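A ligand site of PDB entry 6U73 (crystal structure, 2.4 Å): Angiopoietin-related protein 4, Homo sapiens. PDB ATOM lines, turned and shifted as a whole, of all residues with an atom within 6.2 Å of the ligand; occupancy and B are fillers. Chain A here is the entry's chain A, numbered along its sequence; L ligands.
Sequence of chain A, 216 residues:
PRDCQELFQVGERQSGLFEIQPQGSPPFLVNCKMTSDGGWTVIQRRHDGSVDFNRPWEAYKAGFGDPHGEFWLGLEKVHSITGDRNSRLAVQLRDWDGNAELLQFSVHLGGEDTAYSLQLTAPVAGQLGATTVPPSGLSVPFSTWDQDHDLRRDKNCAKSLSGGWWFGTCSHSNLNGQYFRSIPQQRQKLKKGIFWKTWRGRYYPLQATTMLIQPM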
ATOM      1  N   LEU A  89      39.652  26.458  10.880  1.00  0.00           N
ATOM      2  CA  LEU A  89      38.796  25.899  11.911  1.00  0.00           C
ATOM      3  C   LEU A  89      38.775  24.388  11.710  1.00  0.00           C
ATOM      4  O   LEU A  89      38.275  23.913  10.691  1.00  0.00           O
ATOM      5  CB  LEU A  89      37.374  26.480  11.828  1.00  0.00           C
ATOM      6  CG  LEU A  89      36.364  25.870  12.801  1.00  0.00           C
ATOM      7  CD1 LEU A  89      36.859  26.031  14.230  1.00  0.00           C
ATOM      8  CD2 LEU A  89      35.001  26.509  12.645  1.00  0.00           C
ATOM      9  N   VAL A  91      37.528  20.616  12.812  1.00  0.00           N
ATOM     10  CA  VAL A  91      36.383  19.975  13.430  1.00  0.00           C
ATOM     11  C   VAL A  91      36.644  18.469  13.403  1.00  0.00           C
ATOM     12  O   VAL A  91      36.776  17.886  12.323  1.00  0.00           O
ATOM     13  CB  VAL A  91      35.065  20.305  12.719  1.00  0.00           C
ATOM     14  CG1 VAL A  91      33.927  19.455  13.292  1.00  0.00           C
ATOM     15  CG2 VAL A  91      34.758  21.813  12.805  1.00  0.00           C
ATOM     16  N   PHE A 105      38.083  23.914   7.760  1.00  0.00           N
ATOM     17  CA  PHE A 105      37.501  24.968   6.915  1.00  0.00           C
ATOM     18  C   PHE A 105      38.196  26.289   7.206  1.00  0.00           C
ATOM     19  O   PHE A 105      38.516  26.582   8.362  1.00  0.00           O
ATOM     20  CB  PHE A 105      36.005  25.166   7.183  1.00  0.00           C
ATOM     21  CG  PHE A 105      35.208  23.903   7.274  1.00  0.00           C
ATOM     22  CD1 PHE A 105      34.747  23.287   6.121  1.00  0.00           C
ATOM     23  CD2 PHE A 105      34.903  23.338   8.505  1.00  0.00           C
ATOM     24  CE1 PHE A 105      34.000  22.115   6.191  1.00  0.00           C
ATOM     25  CE2 PHE A 105      34.168  22.169   8.582  1.00  0.00           C
ATOM     26  CZ  PHE A 105      33.716  21.541   7.416  1.00  0.00           C
ATOM     27  N   VAL A 107      37.749  30.093   7.813  1.00  0.00           N
ATOM     28  CA  VAL A 107      36.658  30.941   8.276  1.00  0.00           C
ATOM     29  C   VAL A 107      37.202  32.291   8.726  1.00  0.00           C
ATOM     30  O   VAL A 107      38.378  32.438   9.033  1.00  0.00           O
ATOM     31  CB  VAL A 107      35.846  30.309   9.436  1.00  0.00           C
ATOM     32  CG1 VAL A 107      35.349  28.924   9.081  1.00  0.00           C
ATOM     33  CG2 VAL A 107      36.697  30.295  10.738  1.00  0.00           C
ATOM     34  N   LEU A 118      29.994  33.400  12.212  1.00  0.00           N
ATOM     35  CA  LEU A 118      30.903  32.737  11.297  1.00  0.00           C
ATOM     36  C   LEU A 118      30.692  33.304   9.907  1.00  0.00           C
ATOM     37  O   LEU A 118      29.561  33.294   9.382  1.00  0.00           O
ATOM     38  CB  LEU A 118      30.666  31.229  11.297  1.00  0.00           C
ATOM     39  CG  LEU A 118      31.623  30.322  12.081  1.00  0.00           C
ATOM     40  CD1 LEU A 118      31.520  28.883  11.589  1.00  0.00           C
ATOM     41  CD2 LEU A 118      33.060  30.817  11.984  1.00  0.00           C
ATOM     42  N   LEU A 120      31.742  32.953   6.002  1.00  0.00           N
ATOM     43  CA  LEU A 120      32.224  31.938   5.092  1.00  0.00           C
ATOM     44  C   LEU A 120      32.222  32.482   3.682  1.00  0.00           C
ATOM     45  O   LEU A 120      31.249  33.108   3.256  1.00  0.00           O
ATOM     46  CB  LEU A 120      31.360  30.689   5.183  1.00  0.00           C
ATOM     47  CG  LEU A 120      31.091  30.223   6.608  1.00  0.00           C
ATOM     48  CD1 LEU A 120      30.054  29.135   6.614  1.00  0.00           C
ATOM     49  CD2 LEU A 120      32.414  29.727   7.261  1.00  0.00           C
ATOM     50  N   ALA A 125      31.321  27.699   2.231  1.00  0.00           N
ATOM     51  CA  ALA A 125      29.914  27.366   2.428  1.00  0.00           C
ATOM     52  C   ALA A 125      29.493  26.249   1.494  1.00  0.00           C
ATOM     53  O   ALA A 125      28.617  25.445   1.836  1.00  0.00           O
ATOM     54  CB  ALA A 125      29.036  28.599   2.206  1.00  0.00           C
ATOM     55  N   LEU A 128      30.489  23.028   3.124  1.00  0.00           N
ATOM     56  CA  LEU A 128      29.577  22.614   4.210  1.00  0.00           C
ATOM     57  C   LEU A 128      28.209  22.223   3.692  1.00  0.00           C
ATOM     58  O   LEU A 128      27.397  21.906   4.499  1.00  0.00           O
ATOM     59  CB  LEU A 128      29.472  23.753   5.205  1.00  0.00           C
ATOM     60  CG  LEU A 128      30.735  24.032   5.969  1.00  0.00           C
ATOM     61  CD1 LEU A 128      30.828  25.485   6.303  1.00  0.00           C
ATOM     62  CD2 LEU A 128      30.781  23.205   7.227  1.00  0.00           C
ATOM     63  N   GLY A 129      27.956  22.297   2.395  1.00  0.00           N
ATOM     64  CA  GLY A 129      26.639  21.871   1.915  1.00  0.00           C
ATOM     65  C   GLY A 129      25.809  22.944   1.248  1.00  0.00           C
ATOM     66  O   GLY A 129      24.832  22.565   0.607  1.00  0.00           O
ATOM     67  N   ALA A 130      26.142  24.207   1.404  1.00  0.00           N
ATOM     68  CA  ALA A 130      25.376  25.281   0.721  1.00  0.00           C
ATOM     69  C   ALA A 130      25.579  25.175  -0.800  1.00  0.00           C
ATOM     70  O   ALA A 130      26.696  25.092  -1.268  1.00  0.00           O
ATOM     71  CB  ALA A 130      25.717  26.617   1.273  1.00  0.00           C
ATOM     72  N   LEU A 138      28.604  33.991   3.090  1.00  0.00           N
ATOM     73  CA  LEU A 138      27.551  33.648   4.030  1.00  0.00           C
ATOM     74  C   LEU A 138      27.975  34.050   5.447  1.00  0.00           C
ATOM     75  O   LEU A 138      29.143  33.916   5.810  1.00  0.00           O
ATOM     76  CB  LEU A 138      27.255  32.137   3.976  1.00  0.00           C
ATOM     77  CG  LEU A 138      26.227  31.528   4.920  1.00  0.00           C
ATOM     78  CD1 LEU A 138      24.879  32.183   4.697  1.00  0.00           C
ATOM     79  CD2 LEU A 138      26.152  30.014   4.700  1.00  0.00           C
ATOM     80  N   VAL A 140      26.789  33.533   9.452  1.00  0.00           N
ATOM     81  CA  VAL A 140      25.878  32.814  10.335  1.00  0.00           C
ATOM     82  C   VAL A 140      26.085  33.250  11.784  1.00  0.00           C
ATOM     83  O   VAL A 140      27.150  32.983  12.368  1.00  0.00           O
ATOM     84  CB  VAL A 140      26.038  31.283  10.215  1.00  0.00           C
ATOM     85  CG1 VAL A 140      25.037  30.581  11.141  1.00  0.00           C
ATOM     86  CG2 VAL A 140      25.856  30.823   8.789  1.00  0.00           C
ATOM     87  N   TRP A 165      25.005  27.467  19.196  1.00  0.00           N
ATOM     88  CA  TRP A 165      25.579  27.025  17.938  1.00  0.00           C
ATOM     89  C   TRP A 165      25.360  28.074  16.859  1.00  0.00           C
ATOM     90  O   TRP A 165      24.525  28.974  16.992  1.00  0.00           O
ATOM     91  CB  TRP A 165      24.997  25.661  17.506  1.00  0.00           C
ATOM     92  CG  TRP A 165      25.834  24.922  16.475  1.00  0.00           C
ATOM     93  CD1 TRP A 165      25.452  24.564  15.230  1.00  0.00           C
ATOM     94  CD2 TRP A 165      27.198  24.476  16.621  1.00  0.00           C
ATOM     95  NE1 TRP A 165      26.465  23.906  14.582  1.00  0.00           N
ATOM     96  CE2 TRP A 165      27.558  23.831  15.419  1.00  0.00           C
ATOM     97  CE3 TRP A 165      28.133  24.534  17.654  1.00  0.00           C
ATOM     98  CZ2 TRP A 165      28.828  23.277  15.204  1.00  0.00           C
ATOM     99  CZ3 TRP A 165      29.409  23.975  17.447  1.00  0.00           C
ATOM    100  CH2 TRP A 165      29.734  23.366  16.235  1.00  0.00           C
ATOM    101  N   TRP A 166      26.149  27.953  15.802  1.00  0.00           N
ATOM    102  CA  TRP A 166      25.918  28.688  14.563  1.00  0.00           C
ATOM    103  C   TRP A 166      24.870  27.912  13.767  1.00  0.00           C
ATOM    104  O   TRP A 166      25.178  27.122  12.878  1.00  0.00           O
ATOM    105  CB  TRP A 166      27.203  28.817  13.783  1.00  0.00           C
ATOM    106  CG  TRP A 166      28.245  29.624  14.454  1.00  0.00           C
ATOM    107  CD1 TRP A 166      28.337  30.983  14.493  1.00  0.00           C
ATOM    108  CD2 TRP A 166      29.383  29.119  15.173  1.00  0.00           C
ATOM    109  NE1 TRP A 166      29.462  31.359  15.193  1.00  0.00           N
ATOM    110  CE2 TRP A 166      30.121  30.223  15.618  1.00  0.00           C
ATOM    111  CE3 TRP A 166      29.844  27.837  15.473  1.00  0.00           C
ATOM    112  CZ2 TRP A 166      31.296  30.099  16.344  1.00  0.00           C
ATOM    113  CZ3 TRP A 166      31.017  27.701  16.208  1.00  0.00           C
ATOM    114  CH2 TRP A 166      31.718  28.828  16.638  1.00  0.00           C
ATOM    115  N   PHE A 167      23.606  28.110  14.134  1.00  0.00           N
ATOM    116  CA  PHE A 167      22.485  27.399  13.518  1.00  0.00           C
ATOM    117  C   PHE A 167      22.152  28.080  12.183  1.00  0.00           C
ATOM    118  O   PHE A 167      21.196  28.844  12.052  1.00  0.00           O
ATOM    119  CB  PHE A 167      21.266  27.401  14.435  1.00  0.00           C
ATOM    120  CG  PHE A 167      21.434  26.593  15.715  1.00  0.00           C
ATOM    121  CD1 PHE A 167      21.580  25.211  15.677  1.00  0.00           C
ATOM    122  CD2 PHE A 167      21.396  27.219  16.957  1.00  0.00           C
ATOM    123  CE1 PHE A 167      21.705  24.481  16.870  1.00  0.00           C
ATOM    124  CE2 PHE A 167      21.518  26.502  18.120  1.00  0.00           C
ATOM    125  CZ  PHE A 167      21.671  25.127  18.080  1.00  0.00           C
ATOM    126  N   GLY A 168      22.999  27.843  11.167  1.00  0.00           N
ATOM    127  CA  GLY A 168      22.748  28.354   9.800  1.00  0.00           C
ATOM    128  C   GLY A 168      21.382  27.833   9.419  1.00  0.00           C
ATOM    129  O   GLY A 168      20.494  28.596   9.108  1.00  0.00           O
ATOM    130  N   THR A 169      21.278  26.524   9.417  1.00  0.00           N
ATOM    131  CA  THR A 169      19.921  25.942   9.437  1.00  0.00           C
ATOM    132  C   THR A 169      19.786  25.288  10.808  1.00  0.00           C
ATOM    133  O   THR A 169      20.714  25.270  11.616  1.00  0.00           O
ATOM    134  CB  THR A 169      19.653  24.887   8.368  1.00  0.00           C
ATOM    135  OG1 THR A 169      20.429  23.744   8.710  1.00  0.00           O
ATOM    136  CG2 THR A 169      19.955  25.336   6.966  1.00  0.00           C
ATOM    137  N   CYS A 170      18.629  24.769  11.090  1.00  0.00           N
ATOM    138  CA  CYS A 170      18.463  24.055  12.342  1.00  0.00           C
ATOM    139  C   CYS A 170      18.700  22.561  12.151  1.00  0.00           C
ATOM    140  O   CYS A 170      18.387  21.786  13.052  1.00  0.00           O
ATOM    141  CB  CYS A 170      17.063  24.329  12.897  1.00  0.00           C
ATOM    142  SG  CYS A 170      16.887  24.351  14.713  1.00  0.00           S
ATOM    143  N   SER A 171      19.302  22.155  11.016  1.00  0.00           N
ATOM    144  CA  SER A 171      19.452  20.757  10.644  1.00  0.00           C
ATOM    145  C   SER A 171      20.852  20.401  10.136  1.00  0.00           C
ATOM    146  O   SER A 171      21.045  19.283   9.656  1.00  0.00           O
ATOM    147  CB  SER A 171      18.441  20.355   9.558  1.00  0.00           C
ATOM    148  OG  SER A 171      17.103  20.622   9.933  1.00  0.00           O
ATOM    149  N   HIS A 172      21.828  21.314  10.204  1.00  0.00           N
ATOM    150  CA  HIS A 172      23.155  21.004   9.678  1.00  0.00           C
ATOM    151  C   HIS A 172      24.046  20.329  10.705  1.00  0.00           C
ATOM    152  O   HIS A 172      24.598  19.244  10.457  1.00  0.00           O
ATOM    153  CB  HIS A 172      23.849  22.281   9.168  1.00  0.00           C
ATOM    154  CG  HIS A 172      25.259  22.047   8.751  1.00  0.00           C
ATOM    155  ND1 HIS A 172      26.321  22.103   9.630  1.00  0.00           N
ATOM    156  CD2 HIS A 172      25.794  21.718   7.545  1.00  0.00           C
ATOM    157  CE1 HIS A 172      27.443  21.835   8.985  1.00  0.00           C
ATOM    158  NE2 HIS A 172      27.153  21.597   7.721  1.00  0.00           N
ATOM    159  N   SER A 173      24.239  20.957  11.860  1.00  0.00           N
ATOM    160  CA  SER A 173      25.107  20.414  12.900  1.00  0.00           C
ATOM    161  C   SER A 173      24.727  21.043  14.226  1.00  0.00           C
ATOM    162  O   SER A 173      24.000  22.035  14.286  1.00  0.00           O
ATOM    163  CB  SER A 173      26.591  20.675  12.610  1.00  0.00           C
ATOM    164  OG  SER A 173      26.790  22.031  12.267  1.00  0.00           O
ATOM    165  N   TRP A 196      26.362  15.931  13.374  1.00  0.00           N
ATOM    166  CA  TRP A 196      26.920  16.569  12.188  1.00  0.00           C
ATOM    167  C   TRP A 196      26.319  15.802  11.003  1.00  0.00           C
ATOM    168  O   TRP A 196      26.745  14.685  10.714  1.00  0.00           O
ATOM    169  CB  TRP A 196      28.442  16.496  12.202  1.00  0.00           C
ATOM    170  CG  TRP A 196      29.098  17.201  11.082  1.00  0.00           C
ATOM    171  CD1 TRP A 196      29.293  16.727   9.822  1.00  0.00           C
ATOM    172  CD2 TRP A 196      29.660  18.520  11.115  1.00  0.00           C
ATOM    173  NE1 TRP A 196      29.945  17.663   9.065  1.00  0.00           N
ATOM    174  CE2 TRP A 196      30.181  18.777   9.828  1.00  0.00           C
ATOM    175  CE3 TRP A 196      29.787  19.506  12.105  1.00  0.00           C
ATOM    176  CZ2 TRP A 196      30.812  19.973   9.503  1.00  0.00           C
ATOM    177  CZ3 TRP A 196      30.411  20.696  11.781  1.00  0.00           C
ATOM    178  CH2 TRP A 196      30.919  20.921  10.485  1.00  0.00           C
ATOM    179  N   LYS A 197      25.222  16.323  10.466  1.00  0.00           N
ATOM    180  CA  LYS A 197      24.367  15.629   9.467  1.00  0.00           C
ATOM    181  C   LYS A 197      25.104  14.896   8.347  1.00  0.00           C
ATOM    182  O   LYS A 197      24.780  13.759   8.111  1.00  0.00           O
ATOM    183  CB  LYS A 197      23.280  16.523   8.898  1.00  0.00           C
ATOM    184  CG  LYS A 197      22.231  15.773   8.077  1.00  0.00           C
ATOM    185  CD  LYS A 197      21.130  16.628   7.548  1.00  0.00           C
ATOM    186  CE  LYS A 197      21.600  17.611   6.500  1.00  0.00           C
ATOM    187  NZ  LYS A 197      20.586  18.660   6.265  1.00  0.00           N
ATOM    188  N   THR A 198      26.057  15.530   7.681  1.00  0.00           N
ATOM    189  CA  THR A 198      26.668  14.927   6.507  1.00  0.00           C
ATOM    190  C   THR A 198      27.643  13.803   6.846  1.00  0.00           C
ATOM    191  O   THR A 198      28.028  13.074   5.939  1.00  0.00           O
ATOM    192  CB  THR A 198      27.384  15.972   5.662  1.00  0.00           C
ATOM    193  OG1 THR A 198      28.459  16.545   6.404  1.00  0.00           O
ATOM    194  CG2 THR A 198      26.419  17.061   5.270  1.00  0.00           C
ATOM    195  N   MET A 211      36.925  20.970  18.504  1.00  0.00           N
ATOM    196  CA  MET A 211      37.034  22.054  17.557  1.00  0.00           C
ATOM    197  C   MET A 211      38.277  22.853  17.900  1.00  0.00           C
ATOM    198  O   MET A 211      38.515  23.149  19.073  1.00  0.00           O
ATOM    199  CB  MET A 211      35.801  22.954  17.584  1.00  0.00           C
ATOM    200  CG  MET A 211      34.494  22.204  17.473  1.00  0.00           C
ATOM    201  SD  MET A 211      33.086  23.319  17.622  1.00  0.00           S
ATOM    202  CE  MET A 211      33.303  24.278  16.116  1.00  0.00           C
HETATM  203  C1  LIG L   1      21.956  21.516   5.594  1.00  0.00           C
HETATM  204  O1  LIG L   1      21.139  21.866   6.495  1.00  0.00           O
HETATM  205  O2  LIG L   1      22.274  20.305   5.471  1.00  0.00           O
HETATM  206  C2  LIG L   1      22.560  22.564   4.654  1.00  0.00           C
HETATM  207  C3  LIG L   1      22.996  23.781   5.474  1.00  0.00           C
HETATM  208  C4  LIG L   1      24.108  24.525   4.724  1.00  0.00           C
HETATM  209  C5  LIG L   1      25.242  24.845   5.681  1.00  0.00           C
HETATM  210  C6  LIG L   1      24.856  26.060   6.534  1.00  0.00           C
HETATM  211  C7  LIG L   1      26.127  26.762   7.016  1.00  0.00           C
HETATM  212  C8  LIG L   1      26.851  25.862   8.015  1.00  0.00           C
HETATM  213  C9  LIG L   1      27.150  26.648   9.295  1.00  0.00           C
HETATM  214  C10 LIG L   1      26.990  25.724  10.502  1.00  0.00           C
HETATM  215  C11 LIG L   1      28.185  25.896  11.425  1.00  0.00           C
HETATM  216  C12 LIG L   1      29.417  25.240  10.804  1.00  0.00           C
HETATM  217  C13 LIG L   1      30.472  25.008  11.883  1.00  0.00           C
HETATM  218  C14 LIG L   1      31.824  24.767  11.219  1.00  0.00           C
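An oxygen (O2) of the ligand lies within salt-bridge range of the side-chain amino group (NZ) of Lys 197 (2.5 Å).
The side-chain hydroxyl (OG1) of Thr 169 sits at hydrogen-bond distance from an oxygen (O1) of the ligand (3.0 Å).
A ring nitrogen (NE2) of His 172 sits at hydrogen-bond distance from the backbone carbonyl oxygen of Leu 128 (3.2 Å).
The side-chain amino group (NZ) of Lys 197 sits close to the backbone carbonyl oxygen (O) of Ser 171 (3.5 Å).
OG of Ser 173 lies within hydrogen-bond range of ND1 of His 172 (2.7 Å).
The side-chain hydroxyl (OG1) of Thr 169 sits at hydrogen-bond distance from the backbone NH (N) of Ser 171 (3.0 Å).
The backbone NH (N) of Leu 120 sits at hydrogen-bond distance from the backbone carbonyl oxygen (O) of Leu 138.
O of His 172 sits at hydrogen-bond distance from N of Lys 197, 3.0 Å away.
N of Ala 130 sits at hydrogen-bond distance from O of Ala 125 (2.8 Å).
N of Leu 89 lies within hydrogen-bond range of O of Phe 105 (2.8 Å).
CD2 of Leu 89 touches C14 of the ligand, 3.9 Å away.
Leu 128 touches the ligand (O to C5, 3.8 Å).
Ala 130 touches the ligand (N to C4, 3.9 Å).
CD2 of Leu 138 touches C7 of the ligand, 3.99 Å away.
Trp 166 touches the ligand (O to C10, 3.3 Å).
Ser 171 touches the ligand (C to O1, 3.9 Å).
His 172 touches the ligand (CD2 to C5, 3.7 Å).
Hydrophobic or aromatic side chains that line the ligand: Leu 89, Leu 138, Trp 166 and His 172.
Nine residues have an atom within 4 Å of the ligand: Leu 89, Leu 128, Ala 130, Leu 138, Trp 166, Thr 169, Ser 171, His 172 and Lys 197.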
